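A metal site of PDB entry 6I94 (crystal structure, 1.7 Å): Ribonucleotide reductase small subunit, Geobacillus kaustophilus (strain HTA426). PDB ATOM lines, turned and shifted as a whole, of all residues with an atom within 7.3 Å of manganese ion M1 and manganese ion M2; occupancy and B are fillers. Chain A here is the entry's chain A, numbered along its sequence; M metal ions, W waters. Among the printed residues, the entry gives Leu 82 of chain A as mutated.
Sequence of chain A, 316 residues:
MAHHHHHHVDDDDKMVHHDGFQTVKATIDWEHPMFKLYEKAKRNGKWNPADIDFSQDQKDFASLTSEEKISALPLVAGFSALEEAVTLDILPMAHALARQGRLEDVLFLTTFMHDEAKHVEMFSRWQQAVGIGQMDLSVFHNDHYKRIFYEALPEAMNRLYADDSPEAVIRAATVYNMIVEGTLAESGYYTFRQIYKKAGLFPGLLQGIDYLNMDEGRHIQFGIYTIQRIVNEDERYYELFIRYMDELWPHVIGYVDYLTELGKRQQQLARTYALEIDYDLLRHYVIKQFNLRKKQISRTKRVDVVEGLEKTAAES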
ATOM      1  N   PHE A  79      16.437 -24.942   9.439  1.00  0.00           N
ATOM      2  CA  PHE A  79      17.253 -23.779   9.724  1.00  0.00           C
ATOM      3  C   PHE A  79      17.872 -23.184   8.457  1.00  0.00           C
ATOM      4  O   PHE A  79      18.021 -21.963   8.365  1.00  0.00           O
ATOM      5  CB  PHE A  79      18.351 -24.111  10.741  1.00  0.00           C
ATOM      6  CG  PHE A  79      18.057 -23.566  12.104  1.00  0.00           C
ATOM      7  CD1 PHE A  79      18.035 -22.185  12.323  1.00  0.00           C
ATOM      8  CD2 PHE A  79      17.784 -24.411  13.154  1.00  0.00           C
ATOM      9  CE1 PHE A  79      17.753 -21.675  13.578  1.00  0.00           C
ATOM     10  CE2 PHE A  79      17.505 -23.906  14.423  1.00  0.00           C
ATOM     11  CZ  PHE A  79      17.483 -22.543  14.634  1.00  0.00           C
ATOM     12  N   LEU A  82      15.228 -21.076   6.987  1.00  0.00           N
ATOM     13  CA  LEU A  82      14.956 -19.920   7.832  1.00  0.00           C
ATOM     14  C   LEU A  82      15.988 -18.838   7.597  1.00  0.00           C
ATOM     15  O   LEU A  82      15.651 -17.674   7.373  1.00  0.00           O
ATOM     16  CB  LEU A  82      14.907 -20.316   9.306  1.00  0.00           C
ATOM     17  CG  LEU A  82      14.474 -19.232  10.316  1.00  0.00           C
ATOM     18  CD1 LEU A  82      13.906 -19.929  11.542  1.00  0.00           C
ATOM     19  CD2 LEU A  82      15.603 -18.369  10.718  1.00  0.00           C
ATOM     20  N   GLU A  83      17.267 -19.220   7.614  1.00  0.00           N
ATOM     21  CA  GLU A  83      18.323 -18.205   7.526  1.00  0.00           C
ATOM     22  C   GLU A  83      18.336 -17.584   6.136  1.00  0.00           C
ATOM     23  O   GLU A  83      18.542 -16.375   5.990  1.00  0.00           O
ATOM     24  CB  GLU A  83      19.674 -18.809   7.875  1.00  0.00           C
ATOM     25  CG  GLU A  83      19.719 -19.472   9.292  1.00  0.00           C
ATOM     26  CD  GLU A  83      19.497 -18.526  10.469  1.00  0.00           C
ATOM     27  OE1 GLU A  83      19.197 -19.048  11.570  1.00  0.00           O
ATOM     28  OE2 GLU A  83      19.628 -17.265  10.328  1.00  0.00           O
ATOM     29  N   VAL A  86      15.312 -15.111   5.963  1.00  0.00           N
ATOM     30  CA  VAL A  86      15.449 -13.866   6.714  1.00  0.00           C
ATOM     31  C   VAL A  86      16.563 -13.001   6.119  1.00  0.00           C
ATOM     32  O   VAL A  86      16.535 -11.769   6.252  1.00  0.00           O
ATOM     33  CB  VAL A  86      15.670 -14.114   8.221  1.00  0.00           C
ATOM     34  CG1 VAL A  86      14.441 -14.757   8.853  1.00  0.00           C
ATOM     35  CG2 VAL A  86      16.960 -14.911   8.517  1.00  0.00           C
ATOM     36  N   THR A  87      17.558 -13.616   5.451  1.00  0.00           N
ATOM     37  CA  THR A  87      18.558 -12.804   4.768  1.00  0.00           C
ATOM     38  C   THR A  87      17.906 -11.976   3.680  1.00  0.00           C
ATOM     39  O   THR A  87      18.158 -10.755   3.560  1.00  0.00           O
ATOM     40  CB  THR A  87      19.667 -13.697   4.156  1.00  0.00           C
ATOM     41  OG1 THR A  87      20.358 -14.393   5.178  1.00  0.00           O
ATOM     42  CG2 THR A  87      20.716 -12.847   3.431  1.00  0.00           C
ATOM     43  N   PHE A 112      22.514  -6.416  10.968  1.00  0.00           N
ATOM     44  CA  PHE A 112      21.478  -7.461  10.994  1.00  0.00           C
ATOM     45  C   PHE A 112      21.550  -8.310   9.730  1.00  0.00           C
ATOM     46  O   PHE A 112      21.605  -9.562   9.792  1.00  0.00           O
ATOM     47  CB  PHE A 112      20.132  -6.755  11.167  1.00  0.00           C
ATOM     48  CG  PHE A 112      18.955  -7.624  11.519  1.00  0.00           C
ATOM     49  CD1 PHE A 112      18.139  -7.285  12.577  1.00  0.00           C
ATOM     50  CD2 PHE A 112      18.586  -8.689  10.744  1.00  0.00           C
ATOM     51  CE1 PHE A 112      17.013  -8.053  12.888  1.00  0.00           C
ATOM     52  CE2 PHE A 112      17.466  -9.444  11.050  1.00  0.00           C
ATOM     53  CZ  PHE A 112      16.681  -9.127  12.110  1.00  0.00           C
ATOM     54  N   ASP A 115      24.797 -10.307   9.545  1.00  0.00           N
ATOM     55  CA  ASP A 115      24.673 -11.464  10.432  1.00  0.00           C
ATOM     56  C   ASP A 115      23.929 -12.613   9.739  1.00  0.00           C
ATOM     57  O   ASP A 115      24.371 -13.770   9.744  1.00  0.00           O
ATOM     58  CB  ASP A 115      23.933 -11.068  11.736  1.00  0.00           C
ATOM     59  CG  ASP A 115      24.717 -10.183  12.645  1.00  0.00           C
ATOM     60  OD1 ASP A 115      25.921  -9.986  12.487  1.00  0.00           O
ATOM     61  OD2 ASP A 115      24.079  -9.663  13.590  1.00  0.00           O
ATOM     62  N   GLU A 116      22.768 -12.317   9.128  1.00  0.00           N
ATOM     63  CA  GLU A 116      21.981 -13.377   8.514  1.00  0.00           C
ATOM     64  C   GLU A 116      22.746 -14.039   7.375  1.00  0.00           C
ATOM     65  O   GLU A 116      22.655 -15.251   7.189  1.00  0.00           O
ATOM     66  CB  GLU A 116      20.663 -12.863   7.948  1.00  0.00           C
ATOM     67  CG  GLU A 116      19.750 -12.209   8.938  1.00  0.00           C
ATOM     68  CD  GLU A 116      19.347 -13.042  10.156  1.00  0.00           C
ATOM     69  OE1 GLU A 116      18.622 -12.485  10.948  1.00  0.00           O
ATOM     70  OE2 GLU A 116      19.710 -14.225  10.314  1.00  0.00           O
ATOM     71  N   ALA A 117      23.517 -13.256   6.602  1.00  0.00           N
ATOM     72  CA  ALA A 117      24.370 -13.863   5.573  1.00  0.00           C
ATOM     73  C   ALA A 117      25.316 -14.899   6.163  1.00  0.00           C
ATOM     74  O   ALA A 117      25.525 -15.998   5.591  1.00  0.00           O
ATOM     75  CB  ALA A 117      25.167 -12.781   4.855  1.00  0.00           C
ATOM     76  N   LYS A 118      25.950 -14.555   7.289  1.00  0.00           N
ATOM     77  CA  LYS A 118      26.846 -15.502   7.953  1.00  0.00           C
ATOM     78  C   LYS A 118      26.082 -16.720   8.437  1.00  0.00           C
ATOM     79  O   LYS A 118      26.629 -17.829   8.486  1.00  0.00           O
ATOM     80  CB  LYS A 118      27.552 -14.791   9.127  1.00  0.00           C
ATOM     81  CG  LYS A 118      28.518 -13.719   8.633  1.00  0.00           C
ATOM     82  CD  LYS A 118      29.514 -13.230   9.742  1.00  0.00           C
ATOM     83  CE  LYS A 118      28.818 -12.618  10.926  1.00  0.00           C
ATOM     84  NZ  LYS A 118      29.870 -12.007  11.824  1.00  0.00           N
ATOM     85  N   HIS A 119      24.840 -16.528   8.894  1.00  0.00           N
ATOM     86  CA  HIS A 119      24.056 -17.672   9.379  1.00  0.00           C
ATOM     87  C   HIS A 119      23.720 -18.635   8.252  1.00  0.00           C
ATOM     88  O   HIS A 119      23.830 -19.857   8.430  1.00  0.00           O
ATOM     89  CB  HIS A 119      22.775 -17.191  10.007  1.00  0.00           C
ATOM     90  CG  HIS A 119      22.985 -16.326  11.199  1.00  0.00           C
ATOM     91  ND1 HIS A 119      21.942 -15.727  11.879  1.00  0.00           N
ATOM     92  CD2 HIS A 119      24.120 -15.903  11.802  1.00  0.00           C
ATOM     93  CE1 HIS A 119      22.431 -14.984  12.854  1.00  0.00           C
ATOM     94  NE2 HIS A 119      23.749 -15.072  12.828  1.00  0.00           N
ATOM     95  N   VAL A 120      23.294 -18.109   7.113  1.00  0.00           N
ATOM     96  CA  VAL A 120      23.099 -18.932   5.895  1.00  0.00           C
ATOM     97  C   VAL A 120      24.380 -19.658   5.551  1.00  0.00           C
ATOM     98  O   VAL A 120      24.375 -20.871   5.194  1.00  0.00           O
ATOM     99  CB  VAL A 120      22.669 -18.036   4.712  1.00  0.00           C
ATOM    100  CG1 VAL A 120      22.636 -18.872   3.388  1.00  0.00           C
ATOM    101  CG2 VAL A 120      21.377 -17.402   4.962  1.00  0.00           C
ATOM    102  N   PHE A 123      25.322 -22.751   7.994  1.00  0.00           N
ATOM    103  CA  PHE A 123      24.621 -24.021   7.792  1.00  0.00           C
ATOM    104  C   PHE A 123      24.997 -24.651   6.457  1.00  0.00           C
ATOM    105  O   PHE A 123      25.071 -25.872   6.350  1.00  0.00           O
ATOM    106  CB  PHE A 123      23.120 -23.837   7.875  1.00  0.00           C
ATOM    107  CG  PHE A 123      22.596 -23.688   9.296  1.00  0.00           C
ATOM    108  CD1 PHE A 123      22.667 -24.730  10.188  1.00  0.00           C
ATOM    109  CD2 PHE A 123      22.023 -22.489   9.717  1.00  0.00           C
ATOM    110  CE1 PHE A 123      22.197 -24.585  11.505  1.00  0.00           C
ATOM    111  CE2 PHE A 123      21.556 -22.345  11.009  1.00  0.00           C
ATOM    112  CZ  PHE A 123      21.644 -23.419  11.901  1.00  0.00           C
ATOM    113  N   TYR A 176       8.442 -11.510  11.455  1.00  0.00           N
ATOM    114  CA  TYR A 176       9.866 -11.746  11.283  1.00  0.00           C
ATOM    115  C   TYR A 176      10.558 -11.924  12.631  1.00  0.00           C
ATOM    116  O   TYR A 176      11.181 -12.964  12.892  1.00  0.00           O
ATOM    117  CB  TYR A 176      10.476 -10.579  10.511  1.00  0.00           C
ATOM    118  CG  TYR A 176      11.890 -10.739  10.024  1.00  0.00           C
ATOM    119  CD1 TYR A 176      12.188 -10.645   8.670  1.00  0.00           C
ATOM    120  CD2 TYR A 176      12.927 -10.924  10.909  1.00  0.00           C
ATOM    121  CE1 TYR A 176      13.482 -10.745   8.222  1.00  0.00           C
ATOM    122  CE2 TYR A 176      14.232 -11.031  10.478  1.00  0.00           C
ATOM    123  CZ  TYR A 176      14.513 -10.936   9.151  1.00  0.00           C
ATOM    124  OH  TYR A 176      15.821 -11.016   8.708  1.00  0.00           O
ATOM    125  N   ASN A 177      10.465 -10.925  13.496  1.00  0.00           N
ATOM    126  CA  ASN A 177      11.324 -10.884  14.686  1.00  0.00           C
ATOM    127  C   ASN A 177      10.734 -11.698  15.826  1.00  0.00           C
ATOM    128  O   ASN A 177      11.478 -12.385  16.541  1.00  0.00           O
ATOM    129  CB  ASN A 177      11.549  -9.444  15.147  1.00  0.00           C
ATOM    130  CG  ASN A 177      12.171  -8.585  14.087  1.00  0.00           C
ATOM    131  OD1 ASN A 177      11.505  -7.823  13.431  1.00  0.00           O
ATOM    132  ND2 ASN A 177      13.465  -8.760  13.895  1.00  0.00           N
ATOM    133  N   GLU A 181      12.054 -15.484  14.242  1.00  0.00           N
ATOM    134  CA  GLU A 181      13.306 -15.493  15.028  1.00  0.00           C
ATOM    135  C   GLU A 181      13.034 -15.742  16.510  1.00  0.00           C
ATOM    136  O   GLU A 181      13.698 -16.583  17.121  1.00  0.00           O
ATOM    137  CB  GLU A 181      14.085 -14.196  14.817  1.00  0.00           C
ATOM    138  CG  GLU A 181      14.377 -13.962  13.317  1.00  0.00           C
ATOM    139  CD  GLU A 181      15.740 -13.409  13.009  1.00  0.00           C
ATOM    140  OE1 GLU A 181      15.947 -12.218  13.195  1.00  0.00           O
ATOM    141  OE2 GLU A 181      16.606 -14.205  12.567  1.00  0.00           O
ATOM    142  N   ALA A 185      13.144 -19.865  15.738  1.00  0.00           N
ATOM    143  CA  ALA A 185      14.594 -19.998  15.716  1.00  0.00           C
ATOM    144  C   ALA A 185      15.133 -20.189  17.128  1.00  0.00           C
ATOM    145  O   ALA A 185      15.959 -21.065  17.378  1.00  0.00           O
ATOM    146  CB  ALA A 185      15.258 -18.790  15.063  1.00  0.00           C
ATOM    147  N   TYR A 189      17.436 -23.384  18.223  1.00  0.00           N
ATOM    148  CA  TYR A 189      18.760 -23.376  18.848  1.00  0.00           C
ATOM    149  C   TYR A 189      18.748 -24.289  20.051  1.00  0.00           C
ATOM    150  O   TYR A 189      19.570 -25.205  20.180  1.00  0.00           O
ATOM    151  CB  TYR A 189      19.180 -21.995  19.378  1.00  0.00           C
ATOM    152  CG  TYR A 189      19.099 -20.874  18.419  1.00  0.00           C
ATOM    153  CD1 TYR A 189      19.239 -21.113  17.070  1.00  0.00           C
ATOM    154  CD2 TYR A 189      18.854 -19.575  18.858  1.00  0.00           C
ATOM    155  CE1 TYR A 189      19.136 -20.118  16.190  1.00  0.00           C
ATOM    156  CE2 TYR A 189      18.757 -18.558  17.977  1.00  0.00           C
ATOM    157  CZ  TYR A 189      18.908 -18.833  16.636  1.00  0.00           C
ATOM    158  OH  TYR A 189      18.812 -17.850  15.704  1.00  0.00           O
ATOM    159  N   LEU A 212      25.575 -17.739  16.379  1.00  0.00           N
ATOM    160  CA  LEU A 212      24.306 -17.321  15.812  1.00  0.00           C
ATOM    161  C   LEU A 212      23.352 -16.847  16.911  1.00  0.00           C
ATOM    162  O   LEU A 212      22.672 -15.830  16.769  1.00  0.00           O
ATOM    163  CB  LEU A 212      23.748 -18.511  15.059  1.00  0.00           C
ATOM    164  CG  LEU A 212      22.583 -18.462  14.170  1.00  0.00           C
ATOM    165  CD1 LEU A 212      22.605 -19.645  13.197  1.00  0.00           C
ATOM    166  CD2 LEU A 212      21.439 -18.560  15.083  1.00  0.00           C
ATOM    167  N   ASP A 215      24.291 -13.364  18.017  1.00  0.00           N
ATOM    168  CA  ASP A 215      23.795 -12.374  17.066  1.00  0.00           C
ATOM    169  C   ASP A 215      22.302 -12.124  17.258  1.00  0.00           C
ATOM    170  O   ASP A 215      21.851 -10.993  17.236  1.00  0.00           O
ATOM    171  CB  ASP A 215      24.024 -12.821  15.615  1.00  0.00           C
ATOM    172  CG  ASP A 215      25.470 -12.939  15.244  1.00  0.00           C
ATOM    173  OD1 ASP A 215      26.352 -12.269  15.845  1.00  0.00           O
ATOM    174  OD2 ASP A 215      25.725 -13.716  14.270  1.00  0.00           O
ATOM    175  N   GLU A 216      21.517 -13.190  17.395  1.00  0.00           N
ATOM    176  CA  GLU A 216      20.079 -13.086  17.351  1.00  0.00           C
ATOM    177  C   GLU A 216      19.527 -12.372  18.576  1.00  0.00           C
ATOM    178  O   GLU A 216      18.455 -11.778  18.506  1.00  0.00           O
ATOM    179  CB  GLU A 216      19.471 -14.467  17.189  1.00  0.00           C
ATOM    180  CG  GLU A 216      19.782 -15.040  15.788  1.00  0.00           C
ATOM    181  CD  GLU A 216      19.084 -14.294  14.663  1.00  0.00           C
ATOM    182  OE1 GLU A 216      18.016 -13.676  14.955  1.00  0.00           O
ATOM    183  OE2 GLU A 216      19.614 -14.343  13.517  1.00  0.00           O
ATOM    184  N   GLY A 217      20.285 -12.339  19.676  1.00  0.00           N
ATOM    185  CA  GLY A 217      19.930 -11.449  20.774  1.00  0.00           C
ATOM    186  C   GLY A 217      19.747 -10.013  20.338  1.00  0.00           C
ATOM    187  O   GLY A 217      18.754  -9.363  20.658  1.00  0.00           O
ATOM    188  N   ARG A 218      20.678  -9.519  19.509  1.00  0.00           N
ATOM    189  CA  ARG A 218      20.537  -8.142  19.004  1.00  0.00           C
ATOM    190  C   ARG A 218      19.329  -8.004  18.105  1.00  0.00           C
ATOM    191  O   ARG A 218      18.596  -7.009  18.188  1.00  0.00           O
ATOM    192  CB  ARG A 218      21.786  -7.716  18.240  1.00  0.00           C
ATOM    193  CG  ARG A 218      23.005  -7.590  19.091  1.00  0.00           C
ATOM    194  CD  ARG A 218      24.120  -6.922  18.307  1.00  0.00           C
ATOM    195  NE  ARG A 218      24.482  -7.705  17.125  1.00  0.00           N
ATOM    196  CZ  ARG A 218      25.311  -8.755  17.156  1.00  0.00           C
ATOM    197  NH1 ARG A 218      25.902  -9.125  18.306  1.00  0.00           N
ATOM    198  NH2 ARG A 218      25.581  -9.420  16.028  1.00  0.00           N
ATOM    199  N   HIS A 219      19.132  -8.965  17.197  1.00  0.00           N
ATOM    200  CA  HIS A 219      18.034  -8.904  16.246  1.00  0.00           C
ATOM    201  C   HIS A 219      16.698  -8.777  16.959  1.00  0.00           C
ATOM    202  O   HIS A 219      15.817  -8.031  16.516  1.00  0.00           O
ATOM    203  CB  HIS A 219      18.029 -10.160  15.381  1.00  0.00           C
ATOM    204  CG  HIS A 219      19.254 -10.299  14.555  1.00  0.00           C
ATOM    205  ND1 HIS A 219      19.396 -11.263  13.570  1.00  0.00           N
ATOM    206  CD2 HIS A 219      20.425  -9.629  14.590  1.00  0.00           C
ATOM    207  CE1 HIS A 219      20.590 -11.159  13.034  1.00  0.00           C
ATOM    208  NE2 HIS A 219      21.243 -10.179  13.636  1.00  0.00           N
ATOM    209  N   ILE A 220      16.524  -9.498  18.051  1.00  0.00           N
ATOM    210  CA  ILE A 220      15.202  -9.460  18.690  1.00  0.00           C
ATOM    211  C   ILE A 220      14.999  -8.118  19.383  1.00  0.00           C
ATOM    212  O   ILE A 220      13.878  -7.617  19.449  1.00  0.00           O
ATOM    213  CB  ILE A 220      15.044 -10.666  19.649  1.00  0.00           C
ATOM    214  CG1 ILE A 220      15.086 -11.960  18.830  1.00  0.00           C
ATOM    215  CG2 ILE A 220      13.704 -10.593  20.366  1.00  0.00           C
ATOM    216  CD1 ILE A 220      15.168 -13.280  19.637  1.00  0.00           C
HETATM  217 MN    MN M   1      19.778 -15.758  11.743  1.00  0.00          MN
HETATM  218 MN    MN M   2      18.041 -12.812  12.978  1.00  0.00          MN
HETATM  219  O   HOH W   1      19.043 -17.129  13.255  1.00  0.00           O
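The side-chain carboxylate (OE2) of Glu 83 binds manganese ion M1 (2.1 Å).
OE2 of Glu 116 binds manganese ion M1.
Manganese ion M1 is bound by water W1.
A ring nitrogen (ND1) of His 119 binds manganese ion M1 (2.2 Å).
Manganese ion M1 is bound by OE2 of Glu 216, 2.3 Å away.
Manganese ion M1 has five donor atoms within binding distance.
Of the 25 residues printed, 5 come within 4 Å of manganese ion M1.
The nearest printed residue that does not touch manganese ion M1 is Val 86 (4.4 Å).
Water W1 lies within hydrogen-bond range of OE1 of Glu 83 (2.6 Å) and OH of Tyr 189 (2.6 Å).
Residues that only touch manganese ion M2: Phe 112.
Within 4 Å of manganese ion M2: Phe 112, Glu 116, Glu 181, Glu 216 and His 219.
The nearest printed residue that does not touch manganese ion M2 is Tyr 176 (4.9 Å).
Manganese ion M2 is bound by OE2 of Glu 181 (2.0 Å), OE1 of Glu 116 (2.1 Å), ND1 of His 219 (2.1 Å), OE1 of Glu 216 (2.2 Å), OE1 of Glu 181 (2.2 Å) and OE2 of Glu 216 (2.3 Å).
A ring nitrogen (NE2) of His 219 sits at hydrogen-bond distance from the side-chain carboxylate (OD2) of Asp 115 (2.9 Å).
OD2 of Asp 215 is in hydrogen-bond range of NE2 of His 119, at 2.8 Å.
N of Glu 181 is in hydrogen-bond range of O of Tyr 176, 3.0 Å away.
O of Glu 116 lies within hydrogen-bond range of OG1 of Thr 87.
The backbone carbonyl oxygen (O) of Glu 83 sits at hydrogen-bond distance from the side-chain hydroxyl (OG1) of Thr 87 (2.8 Å).
A ring nitrogen (NE2) of His 119 lies close to the backbone carbonyl oxygen of Asp 115.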
